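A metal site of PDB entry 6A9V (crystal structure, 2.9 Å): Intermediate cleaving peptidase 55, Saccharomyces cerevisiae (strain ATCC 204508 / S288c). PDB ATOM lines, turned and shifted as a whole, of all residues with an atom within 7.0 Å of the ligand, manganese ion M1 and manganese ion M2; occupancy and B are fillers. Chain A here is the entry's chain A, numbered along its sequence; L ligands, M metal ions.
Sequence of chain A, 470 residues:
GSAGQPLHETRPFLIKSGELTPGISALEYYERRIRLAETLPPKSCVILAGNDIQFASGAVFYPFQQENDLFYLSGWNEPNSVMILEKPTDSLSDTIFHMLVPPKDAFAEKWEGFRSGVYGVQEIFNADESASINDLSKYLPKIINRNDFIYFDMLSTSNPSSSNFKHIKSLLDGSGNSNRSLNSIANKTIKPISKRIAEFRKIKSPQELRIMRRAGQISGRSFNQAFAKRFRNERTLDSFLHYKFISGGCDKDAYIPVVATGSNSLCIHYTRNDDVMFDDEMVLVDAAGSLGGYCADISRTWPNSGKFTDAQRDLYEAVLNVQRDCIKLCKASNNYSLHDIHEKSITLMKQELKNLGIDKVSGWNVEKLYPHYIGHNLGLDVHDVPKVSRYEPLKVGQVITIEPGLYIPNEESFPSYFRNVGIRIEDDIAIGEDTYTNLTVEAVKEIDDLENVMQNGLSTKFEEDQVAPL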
ATOM      1  N   TYR A 255       4.074  -7.171 -15.884  1.00  0.00           N
ATOM      2  CA  TYR A 255       3.384  -6.069 -15.235  1.00  0.00           C
ATOM      3  C   TYR A 255       4.383  -4.947 -15.029  1.00  0.00           C
ATOM      4  O   TYR A 255       5.595  -5.124 -15.199  1.00  0.00           O
ATOM      5  CB  TYR A 255       2.770  -6.510 -13.893  1.00  0.00           C
ATOM      6  CG  TYR A 255       3.734  -7.274 -13.014  1.00  0.00           C
ATOM      7  CD1 TYR A 255       3.792  -8.663 -13.059  1.00  0.00           C
ATOM      8  CD2 TYR A 255       4.596  -6.612 -12.157  1.00  0.00           C
ATOM      9  CE1 TYR A 255       4.674  -9.360 -12.267  1.00  0.00           C
ATOM     10  CE2 TYR A 255       5.481  -7.300 -11.361  1.00  0.00           C
ATOM     11  CZ  TYR A 255       5.525  -8.677 -11.415  1.00  0.00           C
ATOM     12  OH  TYR A 255       6.404  -9.377 -10.615  1.00  0.00           O
ATOM     13  N   ILE A 256       3.874  -3.780 -14.647  1.00  0.00           N
ATOM     14  CA  ILE A 256       4.716  -2.621 -14.360  1.00  0.00           C
ATOM     15  C   ILE A 256       5.521  -2.912 -13.098  1.00  0.00           C
ATOM     16  O   ILE A 256       4.938  -3.185 -12.035  1.00  0.00           O
ATOM     17  CB  ILE A 256       3.877  -1.346 -14.230  1.00  0.00           C
ATOM     18  CG1 ILE A 256       3.226  -0.990 -15.573  1.00  0.00           C
ATOM     19  CG2 ILE A 256       4.733  -0.190 -13.722  1.00  0.00           C
ATOM     20  CD1 ILE A 256       2.244   0.152 -15.505  1.00  0.00           C
ATOM     21  N   VAL A 258       8.145  -2.850  -9.744  1.00  0.00           N
ATOM     22  CA  VAL A 258       8.373  -2.047  -8.545  1.00  0.00           C
ATOM     23  C   VAL A 258       9.841  -2.206  -8.155  1.00  0.00           C
ATOM     24  O   VAL A 258      10.308  -3.336  -7.948  1.00  0.00           O
ATOM     25  CB  VAL A 258       7.459  -2.485  -7.391  1.00  0.00           C
ATOM     26  CG1 VAL A 258       7.780  -1.689  -6.131  1.00  0.00           C
ATOM     27  CG2 VAL A 258       5.997  -2.335  -7.772  1.00  0.00           C
ATOM     28  N   VAL A 285      11.939  -5.400  -4.915  1.00  0.00           N
ATOM     29  CA  VAL A 285      11.763  -5.471  -6.358  1.00  0.00           C
ATOM     30  C   VAL A 285      10.663  -6.480  -6.671  1.00  0.00           C
ATOM     31  O   VAL A 285      10.777  -7.659  -6.338  1.00  0.00           O
ATOM     32  CB  VAL A 285      13.055  -5.865  -7.083  1.00  0.00           C
ATOM     33  CG1 VAL A 285      12.782  -6.065  -8.571  1.00  0.00           C
ATOM     34  CG2 VAL A 285      14.111  -4.787  -6.891  1.00  0.00           C
ATOM     35  N   ASP A 286       9.600  -5.998  -7.322  1.00  0.00           N
ATOM     36  CA  ASP A 286       8.530  -6.851  -7.830  1.00  0.00           C
ATOM     37  C   ASP A 286       8.534  -6.720  -9.351  1.00  0.00           C
ATOM     38  O   ASP A 286       8.145  -5.666  -9.888  1.00  0.00           O
ATOM     39  CB  ASP A 286       7.177  -6.445  -7.244  1.00  0.00           C
ATOM     40  CG  ASP A 286       6.124  -7.531  -7.383  1.00  0.00           C
ATOM     41  OD1 ASP A 286       6.166  -8.282  -8.379  1.00  0.00           O
ATOM     42  OD2 ASP A 286       5.249  -7.634  -6.498  1.00  0.00           O
ATOM     43  N   ALA A 287       8.986  -7.763 -10.038  1.00  0.00           N
ATOM     44  CA  ALA A 287       9.120  -7.739 -11.485  1.00  0.00           C
ATOM     45  C   ALA A 287       9.266  -9.166 -11.989  1.00  0.00           C
ATOM     46  O   ALA A 287       9.837 -10.020 -11.301  1.00  0.00           O
ATOM     47  CB  ALA A 287      10.306  -6.885 -11.937  1.00  0.00           C
ATOM     48  N   ALA A 296       4.697 -14.560 -15.102  1.00  0.00           N
ATOM     49  CA  ALA A 296       5.320 -14.873 -13.828  1.00  0.00           C
ATOM     50  C   ALA A 296       5.146 -13.689 -12.883  1.00  0.00           C
ATOM     51  O   ALA A 296       4.699 -12.616 -13.281  1.00  0.00           O
ATOM     52  CB  ALA A 296       6.790 -15.228 -14.008  1.00  0.00           C
ATOM     53  N   ASP A 297       5.512 -13.889 -11.618  1.00  0.00           N
ATOM     54  CA  ASP A 297       5.369 -12.833 -10.630  1.00  0.00           C
ATOM     55  C   ASP A 297       6.342 -13.105  -9.488  1.00  0.00           C
ATOM     56  O   ASP A 297       6.155 -14.057  -8.736  1.00  0.00           O
ATOM     57  CB  ASP A 297       3.926 -12.765 -10.125  1.00  0.00           C
ATOM     58  CG  ASP A 297       3.620 -11.460  -9.420  1.00  0.00           C
ATOM     59  OD1 ASP A 297       4.548 -10.650  -9.230  1.00  0.00           O
ATOM     60  OD2 ASP A 297       2.435 -11.246  -9.063  1.00  0.00           O
ATOM     61  N   ILE A 298       7.363 -12.254  -9.353  1.00  0.00           N
ATOM     62  CA  ILE A 298       8.440 -12.465  -8.390  1.00  0.00           C
ATOM     63  C   ILE A 298       8.660 -11.180  -7.604  1.00  0.00           C
ATOM     64  O   ILE A 298       8.701 -10.089  -8.181  1.00  0.00           O
ATOM     65  CB  ILE A 298       9.740 -12.903  -9.088  1.00  0.00           C
ATOM     66  CG1 ILE A 298       9.570 -14.283  -9.718  1.00  0.00           C
ATOM     67  CG2 ILE A 298      10.911 -12.907  -8.103  1.00  0.00           C
ATOM     68  CD1 ILE A 298      10.805 -14.787 -10.444  1.00  0.00           C
ATOM     69  N   SER A 299       8.805 -11.318  -6.290  1.00  0.00           N
ATOM     70  CA  SER A 299       9.266 -10.232  -5.426  1.00  0.00           C
ATOM     71  C   SER A 299      10.496 -10.699  -4.658  1.00  0.00           C
ATOM     72  O   SER A 299      10.560 -11.848  -4.212  1.00  0.00           O
ATOM     73  CB  SER A 299       8.190  -9.772  -4.439  1.00  0.00           C
ATOM     74  OG  SER A 299       7.051  -9.269  -5.128  1.00  0.00           O
ATOM     75  N   ILE A 374      -2.410 -12.683   0.750  1.00  0.00           N
ATOM     76  CA  ILE A 374      -1.264 -13.597   0.679  1.00  0.00           C
ATOM     77  C   ILE A 374      -0.822 -13.807  -0.765  1.00  0.00           C
ATOM     78  O   ILE A 374       0.364 -14.026  -1.032  1.00  0.00           O
ATOM     79  CB  ILE A 374      -1.597 -14.924   1.373  1.00  0.00           C
ATOM     80  CG1 ILE A 374      -0.368 -15.832   1.435  1.00  0.00           C
ATOM     81  CG2 ILE A 374      -2.736 -15.641   0.654  1.00  0.00           C
ATOM     82  CD1 ILE A 374       0.829 -15.188   2.106  1.00  0.00           C
ATOM     83  N   GLY A 375      -1.755 -13.752  -1.707  1.00  0.00           N
ATOM     84  CA  GLY A 375      -1.416 -14.018  -3.083  1.00  0.00           C
ATOM     85  C   GLY A 375      -2.638 -13.988  -3.969  1.00  0.00           C
ATOM     86  O   GLY A 375      -3.692 -13.455  -3.595  1.00  0.00           O
ATOM     87  N   HIS A 376      -2.496 -14.579  -5.157  1.00  0.00           N
ATOM     88  CA  HIS A 376      -3.538 -14.505  -6.171  1.00  0.00           C
ATOM     89  C   HIS A 376      -3.287 -15.599  -7.199  1.00  0.00           C
ATOM     90  O   HIS A 376      -2.169 -16.085  -7.370  1.00  0.00           O
ATOM     91  CB  HIS A 376      -3.558 -13.137  -6.846  1.00  0.00           C
ATOM     92  CG  HIS A 376      -2.208 -12.689  -7.339  1.00  0.00           C
ATOM     93  ND1 HIS A 376      -1.710 -13.059  -8.563  1.00  0.00           N
ATOM     94  CD2 HIS A 376      -1.268 -11.902  -6.767  1.00  0.00           C
ATOM     95  CE1 HIS A 376      -0.511 -12.523  -8.733  1.00  0.00           C
ATOM     96  NE2 HIS A 376      -0.222 -11.817  -7.651  1.00  0.00           N
ATOM     97  N   LEU A 378      -2.600 -17.033 -10.821  1.00  0.00           N
ATOM     98  CA  LEU A 378      -1.678 -16.535 -11.831  1.00  0.00           C
ATOM     99  C   LEU A 378      -1.879 -17.301 -13.130  1.00  0.00           C
ATOM    100  O   LEU A 378      -2.106 -18.515 -13.118  1.00  0.00           O
ATOM    101  CB  LEU A 378      -0.229 -16.673 -11.357  1.00  0.00           C
ATOM    102  CG  LEU A 378       0.846 -15.985 -12.196  1.00  0.00           C
ATOM    103  CD1 LEU A 378       0.712 -14.473 -12.108  1.00  0.00           C
ATOM    104  CD2 LEU A 378       2.227 -16.430 -11.747  1.00  0.00           C
ATOM    105  N   VAL A 382      -1.971 -11.214 -14.590  1.00  0.00           N
ATOM    106  CA  VAL A 382      -1.215 -11.212 -13.336  1.00  0.00           C
ATOM    107  C   VAL A 382      -2.123 -11.639 -12.185  1.00  0.00           C
ATOM    108  O   VAL A 382      -1.862 -12.629 -11.488  1.00  0.00           O
ATOM    109  CB  VAL A 382      -0.598  -9.836 -13.067  1.00  0.00           C
ATOM    110  CG1 VAL A 382       0.344  -9.897 -11.873  1.00  0.00           C
ATOM    111  CG2 VAL A 382       0.141  -9.333 -14.295  1.00  0.00           C
ATOM    112  N   HIS A 383      -3.212 -10.897 -11.980  1.00  0.00           N
ATOM    113  CA  HIS A 383      -4.268 -11.321 -11.071  1.00  0.00           C
ATOM    114  C   HIS A 383      -5.272 -12.118 -11.887  1.00  0.00           C
ATOM    115  O   HIS A 383      -6.323 -11.623 -12.321  1.00  0.00           O
ATOM    116  CB  HIS A 383      -4.907 -10.116 -10.381  1.00  0.00           C
ATOM    117  CG  HIS A 383      -3.948  -9.316  -9.555  1.00  0.00           C
ATOM    118  ND1 HIS A 383      -4.313  -8.172  -8.874  1.00  0.00           N
ATOM    119  CD2 HIS A 383      -2.630  -9.502  -9.295  1.00  0.00           C
ATOM    120  CE1 HIS A 383      -3.267  -7.691  -8.235  1.00  0.00           C
ATOM    121  NE2 HIS A 383      -2.233  -8.478  -8.467  1.00  0.00           N
ATOM    122  N   THR A 401       0.262 -17.306  -6.191  1.00  0.00           N
ATOM    123  CA  THR A 401       1.461 -16.735  -5.610  1.00  0.00           C
ATOM    124  C   THR A 401       1.364 -16.742  -4.097  1.00  0.00           C
ATOM    125  O   THR A 401       0.277 -16.760  -3.517  1.00  0.00           O
ATOM    126  CB  THR A 401       1.666 -15.295  -6.100  1.00  0.00           C
ATOM    127  OG1 THR A 401       0.626 -14.453  -5.580  1.00  0.00           O
ATOM    128  CG2 THR A 401       1.624 -15.231  -7.620  1.00  0.00           C
ATOM    129  N   ILE A 402       2.525 -16.755  -3.441  1.00  0.00           N
ATOM    130  CA  ILE A 402       2.630 -16.667  -1.991  1.00  0.00           C
ATOM    131  C   ILE A 402       3.551 -15.484  -1.701  1.00  0.00           C
ATOM    132  O   ILE A 402       4.774 -15.612  -1.835  1.00  0.00           O
ATOM    133  CB  ILE A 402       3.169 -17.959  -1.365  1.00  0.00           C
ATOM    134  CG1 ILE A 402       2.282 -19.155  -1.742  1.00  0.00           C
ATOM    135  CG2 ILE A 402       3.262 -17.818   0.151  1.00  0.00           C
ATOM    136  CD1 ILE A 402       0.928 -19.147  -1.063  1.00  0.00           C
ATOM    137  N   GLU A 403       2.977 -14.353  -1.311  1.00  0.00           N
ATOM    138  CA  GLU A 403       3.729 -13.107  -1.162  1.00  0.00           C
ATOM    139  C   GLU A 403       3.346 -12.379   0.114  1.00  0.00           C
ATOM    140  O   GLU A 403       2.688 -11.346   0.088  1.00  0.00           O
ATOM    141  CB  GLU A 403       3.521 -12.209  -2.389  1.00  0.00           C
ATOM    142  CG  GLU A 403       2.072 -12.087  -2.836  1.00  0.00           C
ATOM    143  CD  GLU A 403       1.915 -11.196  -4.049  1.00  0.00           C
ATOM    144  OE1 GLU A 403       1.089 -11.533  -4.929  1.00  0.00           O
ATOM    145  OE2 GLU A 403       2.632 -10.183  -4.132  1.00  0.00           O
ATOM    146  N   ARG A 424       9.145  -7.890   1.008  1.00  0.00           N
ATOM    147  CA  ARG A 424       8.194  -8.827   0.443  1.00  0.00           C
ATOM    148  C   ARG A 424       8.942  -9.904  -0.336  1.00  0.00           C
ATOM    149  O   ARG A 424       9.897  -9.598  -1.056  1.00  0.00           O
ATOM    150  CB  ARG A 424       7.160  -8.137  -0.469  1.00  0.00           C
ATOM    151  CG  ARG A 424       6.128  -9.102  -1.050  1.00  0.00           C
ATOM    152  CD  ARG A 424       4.932  -8.396  -1.676  1.00  0.00           C
ATOM    153  NE  ARG A 424       5.262  -7.751  -2.947  1.00  0.00           N
ATOM    154  CZ  ARG A 424       5.310  -6.431  -3.118  1.00  0.00           C
ATOM    155  NH1 ARG A 424       5.052  -5.615  -2.105  1.00  0.00           N
ATOM    156  NH2 ARG A 424       5.616  -5.928  -4.302  1.00  0.00           N
ATOM    157  N   GLU A 426       8.015 -13.107  -2.895  1.00  0.00           N
ATOM    158  CA  GLU A 426       6.940 -13.692  -3.694  1.00  0.00           C
ATOM    159  C   GLU A 426       7.481 -14.792  -4.584  1.00  0.00           C
ATOM    160  O   GLU A 426       8.510 -14.618  -5.250  1.00  0.00           O
ATOM    161  CB  GLU A 426       6.262 -12.614  -4.543  1.00  0.00           C
ATOM    162  CG  GLU A 426       5.170 -13.139  -5.446  1.00  0.00           C
ATOM    163  CD  GLU A 426       4.427 -12.034  -6.166  1.00  0.00           C
ATOM    164  OE1 GLU A 426       4.995 -10.929  -6.324  1.00  0.00           O
ATOM    165  OE2 GLU A 426       3.266 -12.265  -6.567  1.00  0.00           O
ATOM    166  N   ASP A 428       5.862 -18.249  -7.208  1.00  0.00           N
ATOM    167  CA  ASP A 428       4.709 -18.776  -7.937  1.00  0.00           C
ATOM    168  C   ASP A 428       4.630 -20.278  -7.711  1.00  0.00           C
ATOM    169  O   ASP A 428       5.544 -21.016  -8.098  1.00  0.00           O
ATOM    170  CB  ASP A 428       4.802 -18.446  -9.418  1.00  0.00           C
ATOM    171  CG  ASP A 428       4.910 -16.961  -9.678  1.00  0.00           C
ATOM    172  OD1 ASP A 428       4.460 -16.189  -8.816  1.00  0.00           O
ATOM    173  OD2 ASP A 428       5.442 -16.567 -10.735  1.00  0.00           O
HETATM  174  N1  LIG L   1       3.015  -7.893  -9.254  1.00  0.00           N
HETATM  175  C1  LIG L   1       1.959  -7.392  -8.391  1.00  0.00           C
HETATM  176  C2  LIG L   1       1.465  -8.418  -7.405  1.00  0.00           C
HETATM  177  O1  LIG L   1       2.155  -8.761  -6.444  1.00  0.00           O
HETATM  178  O2  LIG L   1       0.358  -8.933  -7.528  1.00  0.00           O
HETATM  179 MN    MN M   1       1.632 -10.970  -7.076  1.00  0.00          MN
HETATM  180 MN    MN M   2       4.237  -9.272  -7.461  1.00  0.00          MN
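A ring nitrogen (NE2) of His 383 sits close to an oxygen (O2) of the ligand (2.8 Å).
The backbone NH (N) of Thr 401 sits at hydrogen-bond distance from the backbone carbonyl oxygen (O) of His 376 (3.0 Å). O of Val 382 sits at hydrogen-bond distance from ND1 of His 376 (3.0 Å). The backbone NH (N) of Glu 426 is in hydrogen-bond range of the backbone carbonyl oxygen (O) of Ser 299, at 3.1 Å. OD1 of Asp 286 lies close to OH of Tyr 255 (2.5 Å). OD2 of Asp 286 lies close to NH2 of Arg 424 (2.8 Å). OD2 of Asp 428 lies within hydrogen-bond range of N of Asp 297. The side-chain carboxylate (OE1) of Glu 403 sits close to the side-chain hydroxyl (OG1) of Thr 401, at 3.0 Å. The backbone NH (N) of Glu 403 is in hydrogen-bond range of the backbone carbonyl oxygen (O) of Ile 374 (2.6 Å).
Merely in contact with the ligand: Tyr 255. Hydrophobic or aromatic side chains within 4 Å of the ligand: Tyr 255, His 376 and His 383.
Residues that only touch manganese ion M1: Thr 401 (3.9 Å). Of the 22 residues printed, 5 come within 4 Å of manganese ion M1. The nearest printed residue that does not touch manganese ion M1 is His 383 (4.8 Å).
Tyr 255 touches manganese ion M2. Ser 299 touches manganese ion M2 (OG to MN, 3.7 Å). Of the 22 residues printed, 6 come within 4 Å of manganese ion M2.
Manganese ion M1 is bound by NE2 of His 376 (2.1 Å), OE2 of Glu 426 (2.1 Å), OD2 of Asp 297 (2.2 Å), OE1 of Glu 403 (2.3 Å), O1 of the ligand (2.4 Å) and O2 of the ligand (2.4 Å). Manganese ion M1 has six donor atoms within binding distance.
Manganese ion M2 is bound by OE1 of Glu 426 (2.1 Å), OD2 of Asp 286 (2.2 Å), OD1 of Asp 297 (2.3 Å), OD1 of Asp 286 (2.4 Å), O1 of the ligand (2.4 Å) and N1 of the ligand (2.6 Å). Manganese ion M2 has six donor atoms within binding distance.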
